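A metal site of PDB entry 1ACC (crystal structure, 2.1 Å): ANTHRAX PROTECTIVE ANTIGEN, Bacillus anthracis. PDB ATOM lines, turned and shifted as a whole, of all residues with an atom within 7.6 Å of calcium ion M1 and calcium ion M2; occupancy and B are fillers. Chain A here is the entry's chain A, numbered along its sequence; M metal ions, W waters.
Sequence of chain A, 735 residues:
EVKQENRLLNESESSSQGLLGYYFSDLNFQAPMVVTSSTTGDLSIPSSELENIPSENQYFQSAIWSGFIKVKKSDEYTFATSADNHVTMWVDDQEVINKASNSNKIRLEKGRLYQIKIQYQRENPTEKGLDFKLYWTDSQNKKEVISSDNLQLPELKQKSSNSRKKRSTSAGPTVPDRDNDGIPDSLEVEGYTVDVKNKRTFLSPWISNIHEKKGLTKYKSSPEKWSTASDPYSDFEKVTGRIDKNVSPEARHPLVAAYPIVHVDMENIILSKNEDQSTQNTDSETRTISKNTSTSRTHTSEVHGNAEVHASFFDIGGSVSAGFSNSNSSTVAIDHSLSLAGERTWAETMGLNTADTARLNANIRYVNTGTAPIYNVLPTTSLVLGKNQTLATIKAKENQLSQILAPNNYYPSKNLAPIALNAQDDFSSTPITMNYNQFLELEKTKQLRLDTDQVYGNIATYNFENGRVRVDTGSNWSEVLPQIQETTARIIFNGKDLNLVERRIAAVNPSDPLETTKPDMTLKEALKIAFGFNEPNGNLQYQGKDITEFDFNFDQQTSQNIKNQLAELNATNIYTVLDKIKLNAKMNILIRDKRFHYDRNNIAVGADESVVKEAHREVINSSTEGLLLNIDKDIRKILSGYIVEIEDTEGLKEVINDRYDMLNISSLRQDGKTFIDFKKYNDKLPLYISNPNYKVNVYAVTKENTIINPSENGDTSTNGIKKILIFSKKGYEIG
Water W1 lies within hydrogen-bond range of OD1 of Asp 185, O of Pro 223, N of Arg 178 and N of Asp 179.
Within 4 Å of calcium ion M1: Asp 179, Asp 181, Glu 188, Ser 222, Lys 225 and Asp 235.
Within 4 Å of calcium ion M2: Asp 177, Asp 179, Asp 181, Ile 183 and Glu 188.
O of Ser 222 is bound to calcium ion M1, at 2.2 Å.
The side-chain carboxylate (OD2) of Asp 179 is bound to calcium ion M1, 2.3 Å away.
The side-chain carboxylate (OD2) of Asp 235 is bound to calcium ion M1 (2.3 Å).
OE1 of Glu 188 is bound to calcium ion M1.
OD2 of Asp 181 is bound to calcium ion M1 (2.3 Å).
The backbone carbonyl oxygen (O) of Lys 225 is bound to calcium ion M1 (2.4 Å).
Slightly farther from calcium ion M1 lies OE2 of Glu 188 (3.0 Å).
OD1 of Asp 235 is in hydrogen-bond range of N of Thr 228, at 2.9 Å.
The backbone NH (N) of Ser 222 sits at hydrogen-bond distance from the side-chain hydroxyl (OG1) of Thr 228 (2.8 Å).
N of Asp 235 is in hydrogen-bond range of O of Trp 226, at 3.1 Å.
The side-chain hydroxyl (OG) of Ser 222 lies within hydrogen-bond range of the backbone NH (N) of Lys 225 (3.3 Å).
NZ of Lys 225 lies within hydrogen-bond range of O of Thr 228, at 3.0 Å.
The side-chain carboxylate (OD1) of Asp 177 lies close to the backbone NH (N) of Asn 180 (3.3 Å).
The backbone NH of Trp 226 lies close to the side-chain carboxylate of Asp 179 (3.4 Å).
The side-chain carboxylate (OD2) of Asp 177 lies within hydrogen-bond range of the backbone NH (N) of Gly 182 (2.7 Å).
Water W1 binds calcium ion M2 (1.9 Å).
The side-chain carboxylate (OD1) of Asp 177 is bound to calcium ion M2 (2.3 Å).
The side-chain carboxylate (OD1) of Asp 181 binds calcium ion M2, at 2.3 Å.
The backbone carbonyl oxygen (O) of Ile 183 is bound to calcium ion M2, 2.4 Å away.
OE2 of Glu 188 is bound to calcium ion M2 (2.4 Å).
The side-chain carboxylate (OD1) of Asp 179 is bound to calcium ion M2 (2.4 Å).
Calcium ion M2 has six donor atoms within binding distance.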
ATOM      1  N   TYR A  22      -0.695 -37.228   5.194  1.00  0.00           N
ATOM      2  CA  TYR A  22       0.103 -37.330   6.401  1.00  0.00           C
ATOM      3  C   TYR A  22      -0.335 -38.636   7.050  1.00  0.00           C
ATOM      4  O   TYR A  22      -1.522 -38.828   7.316  1.00  0.00           O
ATOM      5  CB  TYR A  22      -0.205 -36.155   7.337  1.00  0.00           C
ATOM      6  CG  TYR A  22       0.192 -34.812   6.770  1.00  0.00           C
ATOM      7  CD1 TYR A  22      -0.643 -34.131   5.896  1.00  0.00           C
ATOM      8  CD2 TYR A  22       1.417 -34.230   7.110  1.00  0.00           C
ATOM      9  CE1 TYR A  22      -0.267 -32.907   5.355  1.00  0.00           C
ATOM     10  CE2 TYR A  22       1.799 -33.003   6.580  1.00  0.00           C
ATOM     11  CZ  TYR A  22       0.955 -32.348   5.701  1.00  0.00           C
ATOM     12  OH  TYR A  22       1.349 -31.148   5.173  1.00  0.00           O
ATOM     13  N   PRO A 176      -0.368 -29.297  11.905  1.00  0.00           N
ATOM     14  CA  PRO A 176       0.418 -28.202  12.489  1.00  0.00           C
ATOM     15  C   PRO A 176       1.530 -27.856  11.534  1.00  0.00           C
ATOM     16  O   PRO A 176       2.530 -28.579  11.429  1.00  0.00           O
ATOM     17  CB  PRO A 176       0.982 -28.822  13.775  1.00  0.00           C
ATOM     18  CG  PRO A 176       0.264 -30.154  13.929  1.00  0.00           C
ATOM     19  CD  PRO A 176       0.028 -30.577  12.517  1.00  0.00           C
ATOM     20  N   ASP A 177       1.359 -26.744  10.842  1.00  0.00           N
ATOM     21  CA  ASP A 177       2.330 -26.300   9.856  1.00  0.00           C
ATOM     22  C   ASP A 177       2.239 -24.781   9.848  1.00  0.00           C
ATOM     23  O   ASP A 177       1.614 -24.179   8.974  1.00  0.00           O
ATOM     24  CB  ASP A 177       1.915 -26.894   8.510  1.00  0.00           C
ATOM     25  CG  ASP A 177       2.861 -26.544   7.383  1.00  0.00           C
ATOM     26  OD1 ASP A 177       3.941 -25.970   7.625  1.00  0.00           O
ATOM     27  OD2 ASP A 177       2.486 -26.841   6.239  1.00  0.00           O
ATOM     28  N   ARG A 178       2.810 -24.174  10.881  1.00  0.00           N
ATOM     29  CA  ARG A 178       2.811 -22.727  11.049  1.00  0.00           C
ATOM     30  C   ARG A 178       3.184 -21.899   9.831  1.00  0.00           C
ATOM     31  O   ARG A 178       2.594 -20.832   9.618  1.00  0.00           O
ATOM     32  CB  ARG A 178       3.705 -22.325  12.232  1.00  0.00           C
ATOM     33  CG  ARG A 178       3.187 -22.744  13.598  1.00  0.00           C
ATOM     34  CD  ARG A 178       4.085 -22.243  14.728  1.00  0.00           C
ATOM     35  NE  ARG A 178       5.390 -22.897  14.757  1.00  0.00           N
ATOM     36  CZ  ARG A 178       5.862 -23.577  15.796  1.00  0.00           C
ATOM     37  NH1 ARG A 178       5.149 -23.677  16.906  1.00  0.00           N
ATOM     38  NH2 ARG A 178       7.061 -24.147  15.732  1.00  0.00           N
ATOM     39  N   ASP A 179       4.151 -22.353   9.035  1.00  0.00           N
ATOM     40  CA  ASP A 179       4.577 -21.590   7.864  1.00  0.00           C
ATOM     41  C   ASP A 179       3.991 -22.014   6.524  1.00  0.00           C
ATOM     42  O   ASP A 179       4.366 -21.491   5.473  1.00  0.00           O
ATOM     43  CB  ASP A 179       6.107 -21.534   7.784  1.00  0.00           C
ATOM     44  CG  ASP A 179       6.745 -22.914   7.718  1.00  0.00           C
ATOM     45  OD1 ASP A 179       6.043 -23.908   7.494  1.00  0.00           O
ATOM     46  OD2 ASP A 179       7.977 -22.989   7.904  1.00  0.00           O
ATOM     47  N   ASN A 180       3.113 -23.017   6.547  1.00  0.00           N
ATOM     48  CA  ASN A 180       2.461 -23.502   5.335  1.00  0.00           C
ATOM     49  C   ASN A 180       3.376 -24.058   4.244  1.00  0.00           C
ATOM     50  O   ASN A 180       3.031 -24.026   3.071  1.00  0.00           O
ATOM     51  CB  ASN A 180       1.564 -22.400   4.760  1.00  0.00           C
ATOM     52  CG  ASN A 180       0.564 -22.925   3.742  1.00  0.00           C
ATOM     53  OD1 ASN A 180       0.456 -22.395   2.639  1.00  0.00           O
ATOM     54  ND2 ASN A 180      -0.193 -23.938   4.129  1.00  0.00           N
ATOM     55  N   ASP A 181       4.547 -24.564   4.620  1.00  0.00           N
ATOM     56  CA  ASP A 181       5.429 -25.154   3.610  1.00  0.00           C
ATOM     57  C   ASP A 181       5.058 -26.616   3.381  1.00  0.00           C
ATOM     58  O   ASP A 181       5.390 -27.198   2.358  1.00  0.00           O
ATOM     59  CB  ASP A 181       6.933 -24.958   3.924  1.00  0.00           C
ATOM     60  CG  ASP A 181       7.361 -25.558   5.270  1.00  0.00           C
ATOM     61  OD1 ASP A 181       6.681 -26.452   5.815  1.00  0.00           O
ATOM     62  OD2 ASP A 181       8.417 -25.116   5.776  1.00  0.00           O
ATOM     63  N   GLY A 182       4.331 -27.191   4.340  1.00  0.00           N
ATOM     64  CA  GLY A 182       3.905 -28.576   4.207  1.00  0.00           C
ATOM     65  C   GLY A 182       4.503 -29.549   5.207  1.00  0.00           C
ATOM     66  O   GLY A 182       3.962 -30.627   5.426  1.00  0.00           O
ATOM     67  N   ILE A 183       5.656 -29.211   5.765  1.00  0.00           N
ATOM     68  CA  ILE A 183       6.310 -30.090   6.729  1.00  0.00           C
ATOM     69  C   ILE A 183       5.795 -29.734   8.125  1.00  0.00           C
ATOM     70  O   ILE A 183       5.790 -28.568   8.506  1.00  0.00           O
ATOM     71  CB  ILE A 183       7.855 -29.910   6.730  1.00  0.00           C
ATOM     72  CG1 ILE A 183       8.394 -29.874   5.301  1.00  0.00           C
ATOM     73  CG2 ILE A 183       8.516 -31.039   7.515  1.00  0.00           C
ATOM     74  CD1 ILE A 183       9.851 -29.478   5.199  1.00  0.00           C
ATOM     75  N   PRO A 184       5.329 -30.741   8.886  1.00  0.00           N
ATOM     76  CA  PRO A 184       4.815 -30.533  10.255  1.00  0.00           C
ATOM     77  C   PRO A 184       5.871 -29.803  11.088  1.00  0.00           C
ATOM     78  O   PRO A 184       7.067 -30.041  10.915  1.00  0.00           O
ATOM     79  CB  PRO A 184       4.611 -31.959  10.751  1.00  0.00           C
ATOM     80  CG  PRO A 184       4.201 -32.675   9.524  1.00  0.00           C
ATOM     81  CD  PRO A 184       5.173 -32.155   8.493  1.00  0.00           C
ATOM     82  N   ASP A 185       5.421 -28.923  11.993  1.00  0.00           N
ATOM     83  CA  ASP A 185       6.340 -28.164  12.835  1.00  0.00           C
ATOM     84  C   ASP A 185       7.290 -29.069  13.600  1.00  0.00           C
ATOM     85  O   ASP A 185       8.468 -28.757  13.766  1.00  0.00           O
ATOM     86  CB  ASP A 185       5.574 -27.322  13.869  1.00  0.00           C
ATOM     87  CG  ASP A 185       4.526 -26.434  13.253  1.00  0.00           C
ATOM     88  OD1 ASP A 185       4.675 -26.053  12.074  1.00  0.00           O
ATOM     89  OD2 ASP A 185       3.561 -26.109  13.962  1.00  0.00           O
ATOM     90  N   SER A 186       6.730 -30.134  14.156  1.00  0.00           N
ATOM     91  CA  SER A 186       7.482 -31.104  14.935  1.00  0.00           C
ATOM     92  C   SER A 186       8.667 -31.683  14.172  1.00  0.00           C
ATOM     93  O   SER A 186       9.776 -31.764  14.700  1.00  0.00           O
ATOM     94  CB  SER A 186       6.555 -32.228  15.417  1.00  0.00           C
ATOM     95  OG  SER A 186       5.775 -32.759  14.360  1.00  0.00           O
ATOM     96  N   GLU A 188      10.238 -30.445  11.448  1.00  0.00           N
ATOM     97  CA  GLU A 188      11.230 -29.431  11.117  1.00  0.00           C
ATOM     98  C   GLU A 188      12.159 -29.211  12.314  1.00  0.00           C
ATOM     99  O   GLU A 188      13.381 -29.183  12.172  1.00  0.00           O
ATOM    100  CB  GLU A 188      10.551 -28.123  10.705  1.00  0.00           C
ATOM    101  CG  GLU A 188       9.847 -28.202   9.355  1.00  0.00           C
ATOM    102  CD  GLU A 188       9.586 -26.837   8.736  1.00  0.00           C
ATOM    103  OE1 GLU A 188      10.513 -26.266   8.125  1.00  0.00           O
ATOM    104  OE2 GLU A 188       8.455 -26.333   8.865  1.00  0.00           O
ATOM    105  N   TYR A 192      14.120 -34.467  10.074  1.00  0.00           N
ATOM    106  CA  TYR A 192      13.394 -35.263   9.116  1.00  0.00           C
ATOM    107  C   TYR A 192      14.317 -35.629   7.971  1.00  0.00           C
ATOM    108  O   TYR A 192      15.458 -35.179   7.910  1.00  0.00           O
ATOM    109  CB  TYR A 192      12.182 -34.480   8.590  1.00  0.00           C
ATOM    110  CG  TYR A 192      12.522 -33.153   7.926  1.00  0.00           C
ATOM    111  CD1 TYR A 192      12.673 -31.987   8.685  1.00  0.00           C
ATOM    112  CD2 TYR A 192      12.660 -33.065   6.547  1.00  0.00           C
ATOM    113  CE1 TYR A 192      12.953 -30.770   8.070  1.00  0.00           C
ATOM    114  CE2 TYR A 192      12.942 -31.854   5.925  1.00  0.00           C
ATOM    115  CZ  TYR A 192      13.081 -30.709   6.686  1.00  0.00           C
ATOM    116  OH  TYR A 192      13.348 -29.528   6.047  1.00  0.00           O
ATOM    117  N   SER A 221      14.756 -27.664   9.807  1.00  0.00           N
ATOM    118  CA  SER A 221      14.432 -26.367   9.252  1.00  0.00           C
ATOM    119  C   SER A 221      13.575 -25.598  10.236  1.00  0.00           C
ATOM    120  O   SER A 221      13.258 -26.093  11.316  1.00  0.00           O
ATOM    121  CB  SER A 221      13.706 -26.554   7.917  1.00  0.00           C
ATOM    122  OG  SER A 221      12.794 -27.648   7.964  1.00  0.00           O
ATOM    123  N   SER A 222      13.307 -24.347   9.907  1.00  0.00           N
ATOM    124  CA  SER A 222      12.494 -23.518  10.774  1.00  0.00           C
ATOM    125  C   SER A 222      11.023 -23.745  10.484  1.00  0.00           C
ATOM    126  O   SER A 222      10.594 -23.696   9.331  1.00  0.00           O
ATOM    127  CB  SER A 222      12.824 -22.044  10.600  1.00  0.00           C
ATOM    128  OG  SER A 222      11.908 -21.249  11.347  1.00  0.00           O
ATOM    129  N   PRO A 223      10.246 -24.054  11.527  1.00  0.00           N
ATOM    130  CA  PRO A 223       8.811 -24.290  11.423  1.00  0.00           C
ATOM    131  C   PRO A 223       8.076 -22.958  11.314  1.00  0.00           C
ATOM    132  O   PRO A 223       6.844 -22.916  11.258  1.00  0.00           O
ATOM    133  CB  PRO A 223       8.496 -24.996  12.735  1.00  0.00           C
ATOM    134  CG  PRO A 223       9.416 -24.301  13.683  1.00  0.00           C
ATOM    135  CD  PRO A 223      10.714 -24.252  12.917  1.00  0.00           C
ATOM    136  N   GLU A 224       8.832 -21.866  11.358  1.00  0.00           N
ATOM    137  CA  GLU A 224       8.275 -20.522  11.265  1.00  0.00           C
ATOM    138  C   GLU A 224       8.610 -19.881   9.937  1.00  0.00           C
ATOM    139  O   GLU A 224       8.097 -18.812   9.613  1.00  0.00           O
ATOM    140  CB  GLU A 224       8.836 -19.620  12.364  1.00  0.00           C
ATOM    141  CG  GLU A 224       9.044 -20.281  13.702  1.00  0.00           C
ATOM    142  CD  GLU A 224       7.769 -20.585  14.451  1.00  0.00           C
ATOM    143  OE1 GLU A 224       6.673 -20.190  14.003  1.00  0.00           O
ATOM    144  OE2 GLU A 224       7.872 -21.229  15.521  1.00  0.00           O
ATOM    145  N   LYS A 225       9.525 -20.485   9.188  1.00  0.00           N
ATOM    146  CA  LYS A 225       9.924 -19.920   7.905  1.00  0.00           C
ATOM    147  C   LYS A 225       9.642 -20.825   6.722  1.00  0.00           C
ATOM    148  O   LYS A 225      10.176 -21.931   6.635  1.00  0.00           O
ATOM    149  CB  LYS A 225      11.392 -19.506   7.930  1.00  0.00           C
ATOM    150  CG  LYS A 225      11.700 -18.394   8.934  1.00  0.00           C
ATOM    151  CD  LYS A 225      13.153 -17.945   8.835  1.00  0.00           C
ATOM    152  CE  LYS A 225      13.395 -17.105   7.588  1.00  0.00           C
ATOM    153  NZ  LYS A 225      14.856 -16.949   7.337  1.00  0.00           N
ATOM    154  N   TRP A 226       8.757 -20.362   5.849  1.00  0.00           N
ATOM    155  CA  TRP A 226       8.381 -21.080   4.646  1.00  0.00           C
ATOM    156  C   TRP A 226       9.672 -21.513   3.922  1.00  0.00           C
ATOM    157  O   TRP A 226       9.766 -22.629   3.428  1.00  0.00           O
ATOM    158  CB  TRP A 226       7.484 -20.199   3.790  1.00  0.00           C
ATOM    159  CG  TRP A 226       7.052 -20.789   2.492  1.00  0.00           C
ATOM    160  CD1 TRP A 226       5.988 -21.630   2.272  1.00  0.00           C
ATOM    161  CD2 TRP A 226       7.645 -20.549   1.217  1.00  0.00           C
ATOM    162  NE1 TRP A 226       5.895 -21.918   0.934  1.00  0.00           N
ATOM    163  CE2 TRP A 226       6.889 -21.267   0.261  1.00  0.00           C
ATOM    164  CE3 TRP A 226       8.744 -19.795   0.782  1.00  0.00           C
ATOM    165  CZ2 TRP A 226       7.206 -21.250  -1.104  1.00  0.00           C
ATOM    166  CZ3 TRP A 226       9.053 -19.777  -0.572  1.00  0.00           C
ATOM    167  CH2 TRP A 226       8.282 -20.504  -1.494  1.00  0.00           C
ATOM    168  N   SER A 227      10.643 -20.615   3.881  1.00  0.00           N
ATOM    169  CA  SER A 227      11.962 -20.894   3.297  1.00  0.00           C
ATOM    170  C   SER A 227      12.902 -20.529   4.426  1.00  0.00           C
ATOM    171  O   SER A 227      12.949 -19.383   4.869  1.00  0.00           O
ATOM    172  CB  SER A 227      12.247 -19.992   2.085  1.00  0.00           C
ATOM    173  OG  SER A 227      13.545 -20.250   1.546  1.00  0.00           O
ATOM    174  N   THR A 228      13.588 -21.511   4.991  1.00  0.00           N
ATOM    175  CA  THR A 228      14.471 -21.224   6.112  1.00  0.00           C
ATOM    176  C   THR A 228      15.656 -20.306   5.778  1.00  0.00           C
ATOM    177  O   THR A 228      16.076 -19.548   6.643  1.00  0.00           O
ATOM    178  CB  THR A 228      14.897 -22.500   6.854  1.00  0.00           C
ATOM    179  OG1 THR A 228      13.735 -23.143   7.379  1.00  0.00           O
ATOM    180  CG2 THR A 228      15.792 -22.145   8.040  1.00  0.00           C
ATOM    181  N   SER A 234      10.570 -23.165  -0.912  1.00  0.00           N
ATOM    182  CA  SER A 234      10.321 -23.629   0.449  1.00  0.00           C
ATOM    183  C   SER A 234      11.115 -24.862   0.859  1.00  0.00           C
ATOM    184  O   SER A 234      11.626 -25.590   0.006  1.00  0.00           O
ATOM    185  CB  SER A 234       8.820 -23.877   0.695  1.00  0.00           C
ATOM    186  OG  SER A 234       8.385 -25.120   0.182  1.00  0.00           O
ATOM    187  N   ASP A 235      11.140 -25.098   2.166  1.00  0.00           N
ATOM    188  CA  ASP A 235      11.855 -26.229   2.740  1.00  0.00           C
ATOM    189  C   ASP A 235      11.342 -27.540   2.161  1.00  0.00           C
ATOM    190  O   ASP A 235      12.108 -28.451   1.871  1.00  0.00           O
ATOM    191  CB  ASP A 235      11.684 -26.220   4.270  1.00  0.00           C
ATOM    192  CG  ASP A 235      12.215 -24.943   4.914  1.00  0.00           C
ATOM    193  OD1 ASP A 235      13.136 -24.317   4.348  1.00  0.00           O
ATOM    194  OD2 ASP A 235      11.703 -24.559   5.986  1.00  0.00           O
ATOM    195  N   PHE A 236      10.017 -27.621   2.005  1.00  0.00           N
ATOM    196  CA  PHE A 236       9.361 -28.795   1.443  1.00  0.00           C
ATOM    197  C   PHE A 236       9.634 -28.928  -0.056  1.00  0.00           C
ATOM    198  O   PHE A 236       9.864 -30.036  -0.553  1.00  0.00           O
ATOM    199  CB  PHE A 236       7.848 -28.732   1.709  1.00  0.00           C
ATOM    200  CG  PHE A 236       7.074 -29.901   1.170  1.00  0.00           C
ATOM    201  CD1 PHE A 236       7.068 -31.129   1.833  1.00  0.00           C
ATOM    202  CD2 PHE A 236       6.318 -29.761   0.006  1.00  0.00           C
ATOM    203  CE1 PHE A 236       6.324 -32.202   1.336  1.00  0.00           C
ATOM    204  CE2 PHE A 236       5.573 -30.833  -0.492  1.00  0.00           C
ATOM    205  CZ  PHE A 236       5.579 -32.052   0.179  1.00  0.00           C
ATOM    206  N   PRO A 254      17.566 -27.050   3.074  1.00  0.00           N
ATOM    207  CA  PRO A 254      16.841 -25.896   3.619  1.00  0.00           C
ATOM    208  C   PRO A 254      17.643 -24.862   4.422  1.00  0.00           C
ATOM    209  O   PRO A 254      17.121 -23.810   4.775  1.00  0.00           O
ATOM    210  CB  PRO A 254      15.736 -26.541   4.455  1.00  0.00           C
ATOM    211  CG  PRO A 254      16.278 -27.901   4.786  1.00  0.00           C
ATOM    212  CD  PRO A 254      16.920 -28.304   3.495  1.00  0.00           C
HETATM  213 CA    CA M   1       9.859 -24.156   7.354  1.00  0.00          CA
HETATM  214 CA    CA M   2       6.208 -26.276   8.100  1.00  0.00          CA
HETATM  215  O   HOH W   1       5.820 -25.309   9.725  1.00  0.00           O
